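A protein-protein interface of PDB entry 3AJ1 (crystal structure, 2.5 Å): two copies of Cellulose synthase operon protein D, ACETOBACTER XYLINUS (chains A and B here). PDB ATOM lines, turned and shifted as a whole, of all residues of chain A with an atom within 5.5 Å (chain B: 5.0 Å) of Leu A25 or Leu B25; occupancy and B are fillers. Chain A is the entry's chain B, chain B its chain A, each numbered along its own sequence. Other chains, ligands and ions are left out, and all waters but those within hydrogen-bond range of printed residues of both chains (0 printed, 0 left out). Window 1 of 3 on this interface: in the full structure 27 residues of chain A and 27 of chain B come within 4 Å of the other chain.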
ATOM      1  N   PHE A  21     -12.912  -9.234  27.885  1.00  0.00           N
ATOM      2  CA  PHE A  21     -12.300 -10.563  27.919  1.00  0.00           C
ATOM      3  C   PHE A  21     -12.185 -11.131  29.320  1.00  0.00           C
ATOM      4  O   PHE A  21     -11.670 -12.234  29.499  1.00  0.00           O
ATOM      5  CB  PHE A  21     -10.920 -10.556  27.278  1.00  0.00           C
ATOM      6  CG  PHE A  21     -10.929 -10.205  25.826  1.00  0.00           C
ATOM      7  CD1 PHE A  21     -11.536 -11.047  24.901  1.00  0.00           C
ATOM      8  CD2 PHE A  21     -10.291  -9.050  25.372  1.00  0.00           C
ATOM      9  CE1 PHE A  21     -11.543 -10.734  23.551  1.00  0.00           C
ATOM     10  CE2 PHE A  21     -10.287  -8.728  24.013  1.00  0.00           C
ATOM     11  CZ  PHE A  21     -10.915  -9.572  23.102  1.00  0.00           C
ATOM     12  N   THR A  22     -12.652 -10.389  30.318  1.00  0.00           N
ATOM     13  CA  THR A  22     -12.632 -10.899  31.687  1.00  0.00           C
ATOM     14  C   THR A  22     -13.352 -12.250  31.878  1.00  0.00           C
ATOM     15  O   THR A  22     -12.785 -13.135  32.493  1.00  0.00           O
ATOM     16  CB  THR A  22     -13.155  -9.861  32.710  1.00  0.00           C
ATOM     17  OG1 THR A  22     -12.611  -8.571  32.406  1.00  0.00           O
ATOM     18  CG2 THR A  22     -12.750 -10.247  34.121  1.00  0.00           C
ATOM     19  N   LEU A  23     -14.578 -12.411  31.375  1.00  0.00           N
ATOM     20  CA  LEU A  23     -15.300 -13.689  31.553  1.00  0.00           C
ATOM     21  C   LEU A  23     -14.598 -14.840  30.823  1.00  0.00           C
ATOM     22  O   LEU A  23     -14.496 -15.949  31.363  1.00  0.00           O
ATOM     23  CB  LEU A  23     -16.778 -13.609  31.139  1.00  0.00           C
ATOM     24  CG  LEU A  23     -17.821 -14.572  31.764  1.00  0.00           C
ATOM     25  CD1 LEU A  23     -17.938 -15.915  31.038  1.00  0.00           C
ATOM     26  CD2 LEU A  23     -17.670 -14.821  33.278  1.00  0.00           C
ATOM     27  N   PHE A  24     -14.088 -14.549  29.620  1.00  0.00           N
ATOM     28  CA  PHE A  24     -13.387 -15.538  28.832  1.00  0.00           C
ATOM     29  C   PHE A  24     -12.134 -16.007  29.585  1.00  0.00           C
ATOM     30  O   PHE A  24     -11.874 -17.206  29.669  1.00  0.00           O
ATOM     31  CB  PHE A  24     -13.056 -14.986  27.444  1.00  0.00           C
ATOM     32  CG  PHE A  24     -11.999 -15.772  26.714  1.00  0.00           C
ATOM     33  CD1 PHE A  24     -12.326 -16.952  26.068  1.00  0.00           C
ATOM     34  CD2 PHE A  24     -10.679 -15.320  26.661  1.00  0.00           C
ATOM     35  CE1 PHE A  24     -11.365 -17.694  25.396  1.00  0.00           C
ATOM     36  CE2 PHE A  24      -9.696 -16.062  25.999  1.00  0.00           C
ATOM     37  CZ  PHE A  24     -10.044 -17.251  25.355  1.00  0.00           C
ATOM     38  N   LEU A  25     -11.385 -15.062  30.154  1.00  0.00           N
ATOM     39  CA  LEU A  25     -10.175 -15.362  30.913  1.00  0.00           C
ATOM     40  C   LEU A  25     -10.432 -16.097  32.240  1.00  0.00           C
ATOM     41  O   LEU A  25      -9.630 -16.933  32.670  1.00  0.00           O
ATOM     42  CB  LEU A  25      -9.376 -14.072  31.145  1.00  0.00           C
ATOM     43  CG  LEU A  25      -8.208 -13.730  30.200  1.00  0.00           C
ATOM     44  CD1 LEU A  25      -8.158 -14.582  28.940  1.00  0.00           C
ATOM     45  CD2 LEU A  25      -8.179 -12.241  29.847  1.00  0.00           C
ATOM     46  N   GLN A  26     -11.538 -15.770  32.900  1.00  0.00           N
ATOM     47  CA  GLN A  26     -11.944 -16.509  34.093  1.00  0.00           C
ATOM     48  C   GLN A  26     -12.122 -17.999  33.799  1.00  0.00           C
ATOM     49  O   GLN A  26     -11.608 -18.853  34.530  1.00  0.00           O
ATOM     50  CB  GLN A  26     -13.239 -15.955  34.638  1.00  0.00           C
ATOM     51  CG  GLN A  26     -13.071 -14.713  35.472  1.00  0.00           C
ATOM     52  CD  GLN A  26     -14.410 -14.155  35.911  1.00  0.00           C
ATOM     53  OE1 GLN A  26     -14.956 -13.264  35.271  1.00  0.00           O
ATOM     54  NE2 GLN A  26     -14.955 -14.699  36.985  1.00  0.00           N
ATOM     55  N   THR A  27     -12.812 -18.286  32.697  1.00  0.00           N
ATOM     56  CA  THR A  27     -13.143 -19.636  32.333  1.00  0.00           C
ATOM     57  C   THR A  27     -11.913 -20.319  31.745  1.00  0.00           C
ATOM     58  O   THR A  27     -11.647 -21.489  32.066  1.00  0.00           O
ATOM     59  CB  THR A  27     -14.344 -19.689  31.384  1.00  0.00           C
ATOM     60  OG1 THR A  27     -14.008 -19.010  30.182  1.00  0.00           O
ATOM     61  CG2 THR A  27     -15.520 -18.965  31.963  1.00  0.00           C
ATOM     62  N   LEU A  28     -11.140 -19.597  30.925  1.00  0.00           N
ATOM     63  CA  LEU A  28      -9.861 -20.139  30.446  1.00  0.00           C
ATOM     64  C   LEU A  28      -8.986 -20.561  31.624  1.00  0.00           C
ATOM     65  O   LEU A  28      -8.450 -21.672  31.623  1.00  0.00           O
ATOM     66  CB  LEU A  28      -9.102 -19.178  29.520  1.00  0.00           C
ATOM     67  CG  LEU A  28      -7.774 -19.686  28.902  1.00  0.00           C
ATOM     68  CD1 LEU A  28      -7.995 -20.894  27.967  1.00  0.00           C
ATOM     69  CD2 LEU A  28      -6.997 -18.606  28.165  1.00  0.00           C
ATOM     70  N   SER A  29      -8.862 -19.700  32.635  1.00  0.00           N
ATOM     71  CA  SER A  29      -7.993 -20.002  33.775  1.00  0.00           C
ATOM     72  C   SER A  29      -8.422 -21.246  34.539  1.00  0.00           C
ATOM     73  O   SER A  29      -7.579 -22.055  34.899  1.00  0.00           O
ATOM     74  CB  SER A  29      -7.886 -18.820  34.734  1.00  0.00           C
ATOM     75  OG  SER A  29      -9.159 -18.457  35.212  1.00  0.00           O
ATOM     76  N   TRP A  30      -9.724 -21.370  34.809  1.00  0.00           N
ATOM     77  CA  TRP A  30     -10.291 -22.564  35.436  1.00  0.00           C
ATOM     78  C   TRP A  30     -10.032 -23.825  34.591  1.00  0.00           C
ATOM     79  O   TRP A  30      -9.627 -24.853  35.127  1.00  0.00           O
ATOM     80  CB  TRP A  30     -11.791 -22.373  35.695  1.00  0.00           C
ATOM     81  CG  TRP A  30     -12.081 -21.753  37.026  1.00  0.00           C
ATOM     82  CD1 TRP A  30     -11.735 -20.507  37.431  1.00  0.00           C
ATOM     83  CD2 TRP A  30     -12.761 -22.361  38.128  1.00  0.00           C
ATOM     84  NE1 TRP A  30     -12.160 -20.289  38.714  1.00  0.00           N
ATOM     85  CE2 TRP A  30     -12.804 -21.409  39.165  1.00  0.00           C
ATOM     86  CE3 TRP A  30     -13.353 -23.616  38.335  1.00  0.00           C
ATOM     87  CZ2 TRP A  30     -13.394 -21.667  40.399  1.00  0.00           C
ATOM     88  CZ3 TRP A  30     -13.949 -23.875  39.580  1.00  0.00           C
ATOM     89  CH2 TRP A  30     -13.958 -22.903  40.589  1.00  0.00           C
ATOM     90  N   VAL A 104      -8.329 -11.974  37.298  1.00  0.00           N
ATOM     91  CA  VAL A 104      -9.181 -12.746  36.394  1.00  0.00           C
ATOM     92  C   VAL A 104      -9.971 -13.820  37.149  1.00  0.00           C
ATOM     93  O   VAL A 104      -9.944 -14.987  36.780  1.00  0.00           O
ATOM     94  CB  VAL A 104      -8.334 -13.439  35.314  1.00  0.00           C
ATOM     95  CG1 VAL A 104      -9.216 -14.116  34.358  1.00  0.00           C
ATOM     96  CG2 VAL A 104      -7.523 -12.443  34.541  1.00  0.00           C
ATOM     97  N   TRP A 114      -3.722 -15.131  39.146  1.00  0.00           N
ATOM     98  CA  TRP A 114      -3.421 -16.051  38.041  1.00  0.00           C
ATOM     99  C   TRP A 114      -2.444 -15.470  36.995  1.00  0.00           C
ATOM    100  O   TRP A 114      -1.546 -16.154  36.496  1.00  0.00           O
ATOM    101  CB  TRP A 114      -4.744 -16.464  37.376  1.00  0.00           C
ATOM    102  CG  TRP A 114      -4.645 -17.636  36.465  1.00  0.00           C
ATOM    103  CD1 TRP A 114      -4.593 -18.957  36.824  1.00  0.00           C
ATOM    104  CD2 TRP A 114      -4.596 -17.610  35.038  1.00  0.00           C
ATOM    105  NE1 TRP A 114      -4.521 -19.752  35.712  1.00  0.00           N
ATOM    106  CE2 TRP A 114      -4.519 -18.959  34.596  1.00  0.00           C
ATOM    107  CE3 TRP A 114      -4.615 -16.587  34.085  1.00  0.00           C
ATOM    108  CZ2 TRP A 114      -4.450 -19.305  33.238  1.00  0.00           C
ATOM    109  CZ3 TRP A 114      -4.563 -16.933  32.727  1.00  0.00           C
ATOM    110  CH2 TRP A 114      -4.480 -18.283  32.318  1.00  0.00           C
ATOM    111  N   PHE B  21      -6.922  -6.639  27.488  1.00  0.00           N
ATOM    112  CA  PHE B  21      -6.358  -7.977  27.335  1.00  0.00           C
ATOM    113  C   PHE B  21      -5.991  -8.351  25.897  1.00  0.00           C
ATOM    114  O   PHE B  21      -5.521  -9.459  25.650  1.00  0.00           O
ATOM    115  CB  PHE B  21      -7.270  -9.030  27.979  1.00  0.00           C
ATOM    116  CG  PHE B  21      -7.386  -8.896  29.470  1.00  0.00           C
ATOM    117  CD1 PHE B  21      -6.304  -9.203  30.299  1.00  0.00           C
ATOM    118  CD2 PHE B  21      -8.582  -8.476  30.054  1.00  0.00           C
ATOM    119  CE1 PHE B  21      -6.402  -9.069  31.682  1.00  0.00           C
ATOM    120  CE2 PHE B  21      -8.689  -8.335  31.449  1.00  0.00           C
ATOM    121  CZ  PHE B  21      -7.599  -8.635  32.259  1.00  0.00           C
ATOM    122  N   THR B  22      -6.172  -7.415  24.966  1.00  0.00           N
ATOM    123  CA  THR B  22      -5.942  -7.666  23.537  1.00  0.00           C
ATOM    124  C   THR B  22      -4.522  -8.150  23.253  1.00  0.00           C
ATOM    125  O   THR B  22      -4.332  -9.125  22.508  1.00  0.00           O
ATOM    126  CB  THR B  22      -6.252  -6.420  22.662  1.00  0.00           C
ATOM    127  OG1 THR B  22      -7.657  -6.127  22.705  1.00  0.00           O
ATOM    128  CG2 THR B  22      -5.858  -6.664  21.199  1.00  0.00           C
ATOM    129  N   LEU B  23      -3.543  -7.472  23.852  1.00  0.00           N
ATOM    130  CA  LEU B  23      -2.126  -7.780  23.653  1.00  0.00           C
ATOM    131  C   LEU B  23      -1.789  -9.108  24.299  1.00  0.00           C
ATOM    132  O   LEU B  23      -1.054  -9.912  23.728  1.00  0.00           O
ATOM    133  CB  LEU B  23      -1.238  -6.686  24.267  1.00  0.00           C
ATOM    134  CG  LEU B  23       0.071  -6.224  23.615  1.00  0.00           C
ATOM    135  CD1 LEU B  23       1.010  -5.727  24.701  1.00  0.00           C
ATOM    136  CD2 LEU B  23       0.765  -7.281  22.769  1.00  0.00           C
ATOM    137  N   PHE B  24      -2.318  -9.325  25.498  1.00  0.00           N
ATOM    138  CA  PHE B  24      -2.186 -10.612  26.171  1.00  0.00           C
ATOM    139  C   PHE B  24      -2.728 -11.751  25.300  1.00  0.00           C
ATOM    140  O   PHE B  24      -2.023 -12.710  25.033  1.00  0.00           O
ATOM    141  CB  PHE B  24      -2.885 -10.611  27.530  1.00  0.00           C
ATOM    142  CG  PHE B  24      -2.753 -11.912  28.265  1.00  0.00           C
ATOM    143  CD1 PHE B  24      -1.523 -12.311  28.772  1.00  0.00           C
ATOM    144  CD2 PHE B  24      -3.849 -12.754  28.424  1.00  0.00           C
ATOM    145  CE1 PHE B  24      -1.393 -13.530  29.441  1.00  0.00           C
ATOM    146  CE2 PHE B  24      -3.724 -13.972  29.087  1.00  0.00           C
ATOM    147  CZ  PHE B  24      -2.498 -14.359  29.599  1.00  0.00           C
ATOM    148  N   LEU B  25      -3.960 -11.615  24.822  1.00  0.00           N
ATOM    149  CA  LEU B  25      -4.572 -12.642  23.987  1.00  0.00           C
ATOM    150  C   LEU B  25      -3.794 -12.856  22.701  1.00  0.00           C
ATOM    151  O   LEU B  25      -3.668 -13.983  22.218  1.00  0.00           O
ATOM    152  CB  LEU B  25      -6.027 -12.308  23.701  1.00  0.00           C
ATOM    153  CG  LEU B  25      -7.088 -12.998  24.556  1.00  0.00           C
ATOM    154  CD1 LEU B  25      -6.530 -13.508  25.849  1.00  0.00           C
ATOM    155  CD2 LEU B  25      -8.228 -12.051  24.811  1.00  0.00           C
ATOM    156  N   GLN B  26      -3.244 -11.778  22.163  1.00  0.00           N
ATOM    157  CA  GLN B  26      -2.475 -11.875  20.940  1.00  0.00           C
ATOM    158  C   GLN B  26      -1.291 -12.779  21.126  1.00  0.00           C
ATOM    159  O   GLN B  26      -1.036 -13.645  20.298  1.00  0.00           O
ATOM    160  CB  GLN B  26      -2.009 -10.509  20.484  1.00  0.00           C
ATOM    161  CG  GLN B  26      -3.012  -9.788  19.617  1.00  0.00           C
ATOM    162  CD  GLN B  26      -2.474  -8.457  19.160  1.00  0.00           C
ATOM    163  OE1 GLN B  26      -2.750  -7.439  19.778  1.00  0.00           O
ATOM    164  NE2 GLN B  26      -1.671  -8.460  18.092  1.00  0.00           N
ATOM    165  N   THR B  27      -0.576 -12.599  22.225  1.00  0.00           N
ATOM    166  CA  THR B  27       0.624 -13.384  22.427  1.00  0.00           C
ATOM    167  C   THR B  27       0.259 -14.734  23.034  1.00  0.00           C
ATOM    168  O   THR B  27       0.988 -15.704  22.856  1.00  0.00           O
ATOM    169  CB  THR B  27       1.724 -12.644  23.264  1.00  0.00           C
ATOM    170  OG1 THR B  27       1.515 -12.897  24.653  1.00  0.00           O
ATOM    171  CG2 THR B  27       1.710 -11.150  23.024  1.00  0.00           C
ATOM    172  N   LEU B  28      -0.867 -14.797  23.746  1.00  0.00           N
ATOM    173  CA  LEU B  28      -1.375 -16.076  24.234  1.00  0.00           C
ATOM    174  C   LEU B  28      -1.751 -16.960  23.033  1.00  0.00           C
ATOM    175  O   LEU B  28      -1.345 -18.119  22.957  1.00  0.00           O
ATOM    176  CB  LEU B  28      -2.558 -15.895  25.186  1.00  0.00           C
ATOM    177  CG  LEU B  28      -3.307 -17.157  25.669  1.00  0.00           C
ATOM    178  CD1 LEU B  28      -2.570 -17.926  26.772  1.00  0.00           C
ATOM    179  CD2 LEU B  28      -4.641 -16.749  26.181  1.00  0.00           C
ATOM    180  N   SER B  29      -2.482 -16.406  22.072  1.00  0.00           N
ATOM    181  CA  SER B  29      -2.819 -17.197  20.891  1.00  0.00           C
ATOM    182  C   SER B  29      -1.574 -17.786  20.193  1.00  0.00           C
ATOM    183  O   SER B  29      -1.615 -18.938  19.732  1.00  0.00           O
ATOM    184  CB  SER B  29      -3.688 -16.412  19.917  1.00  0.00           C
ATOM    185  OG  SER B  29      -2.905 -15.484  19.193  1.00  0.00           O
ATOM    186  N   TRP B  30      -0.477 -17.025  20.128  1.00  0.00           N
ATOM    187  CA  TRP B  30       0.734 -17.507  19.447  1.00  0.00           C
ATOM    188  C   TRP B  30       1.427 -18.612  20.225  1.00  0.00           C
ATOM    189  O   TRP B  30       1.872 -19.603  19.649  1.00  0.00           O
ATOM    190  CB  TRP B  30       1.729 -16.371  19.185  1.00  0.00           C
ATOM    191  CG  TRP B  30       1.507 -15.665  17.902  1.00  0.00           C
ATOM    192  CD1 TRP B  30       0.371 -15.005  17.504  1.00  0.00           C
ATOM    193  CD2 TRP B  30       2.448 -15.525  16.832  1.00  0.00           C
ATOM    194  NE1 TRP B  30       0.547 -14.473  16.246  1.00  0.00           N
ATOM    195  CE2 TRP B  30       1.813 -14.775  15.811  1.00  0.00           C
ATOM    196  CE3 TRP B  30       3.763 -15.971  16.630  1.00  0.00           C
ATOM    197  CZ2 TRP B  30       2.450 -14.457  14.616  1.00  0.00           C
ATOM    198  CZ3 TRP B  30       4.397 -15.651  15.432  1.00  0.00           C
ATOM    199  CH2 TRP B  30       3.737 -14.901  14.446  1.00  0.00           C
ATOM    200  N   VAL B 104      -8.154 -10.970  17.605  1.00  0.00           N
ATOM    201  CA  VAL B 104      -7.090 -11.232  18.570  1.00  0.00           C
ATOM    202  C   VAL B 104      -5.777 -11.388  17.817  1.00  0.00           C
ATOM    203  O   VAL B 104      -5.039 -12.360  18.013  1.00  0.00           O
ATOM    204  CB  VAL B 104      -7.342 -12.545  19.340  1.00  0.00           C
ATOM    205  CG1 VAL B 104      -6.503 -12.599  20.569  1.00  0.00           C
ATOM    206  CG2 VAL B 104      -8.777 -12.670  19.737  1.00  0.00           C
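Of chain B, only Phe B21 and Leu B25 come within 4 Å of Leu A25. Printed residues of chain A within 4 Å of Phe B21: Phe A21 and Leu A25. Of the printed residues of chain A, Thr B22 touches Phe A21. Of chain A, only Phe A21 (3.4 Å) and Leu A25 (3.7 Å) come within 4 Å of Leu B25. The nearest residue of chain B that does not touch Leu A25 is Phe B24 (4.5 Å). The nearest residue of chain A that does not touch Leu B25 is Phe A24 (4.1 Å). The nearest printed residue of chain B that does not touch Phe A21 is Val B104 (5.0 Å).
Among the printed residues, pairs that only touch across the chains: Phe A21 with Leu B25 (3.4 Å), Leu A25 with Phe B21 (3.5 Å), Leu A28 with Leu B28 (3.6 Å), Leu A25 with Leu B25 (3.7 Å), Phe A21 with Thr B22 (3.9 Å) and Phe A21 with Phe B21 (3.99 Å).
Phe B21 touches its own counterpart, Phe A21. Phe A21 touches Leu B25, and with the chains exchanged Leu A25 touches Phe B21. Leu A25 touches its own counterpart, Leu B25. Leu B28 touches its own counterpart, Leu A28. Positions printed for both chains: 21, 22, 23, 24, 25, 26, 27, 28, 29, 30 and 104. Of the 6 pairs that touch across the chains among the printed residues, 5 have their exchanged pair printed and touching as well.
The backbone carbonyl oxygen (O) of Leu B25 sits close to the side-chain hydroxyl (OG) of Ser B29 (3.5 Å). The side-chain hydroxyl of Ser A29 is in hydrogen-bond range of the backbone carbonyl oxygen of Leu A25 (3.0 Å).
Hydrophobic or aromatic side chains of chain A that line the printed part of chain B: Phe A21, Leu A25 and Leu A28. Along chain A the printed residues that touch a printed residue of chain B span positions 21 to 28. Of the 11 printed residues of chain B, 4 touch a printed residue of chain A. Printed residues of chain B that touch a printed residue of chain A: Phe B21, Thr B22, Leu B25 and Leu B28. Along chain B the printed residues that touch a printed residue of chain A span positions 21 to 28. Among the printed residues, no Asp or Glu carboxylate lies within 4 Å of a Lys or Arg side-chain nitrogen of the other chain.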
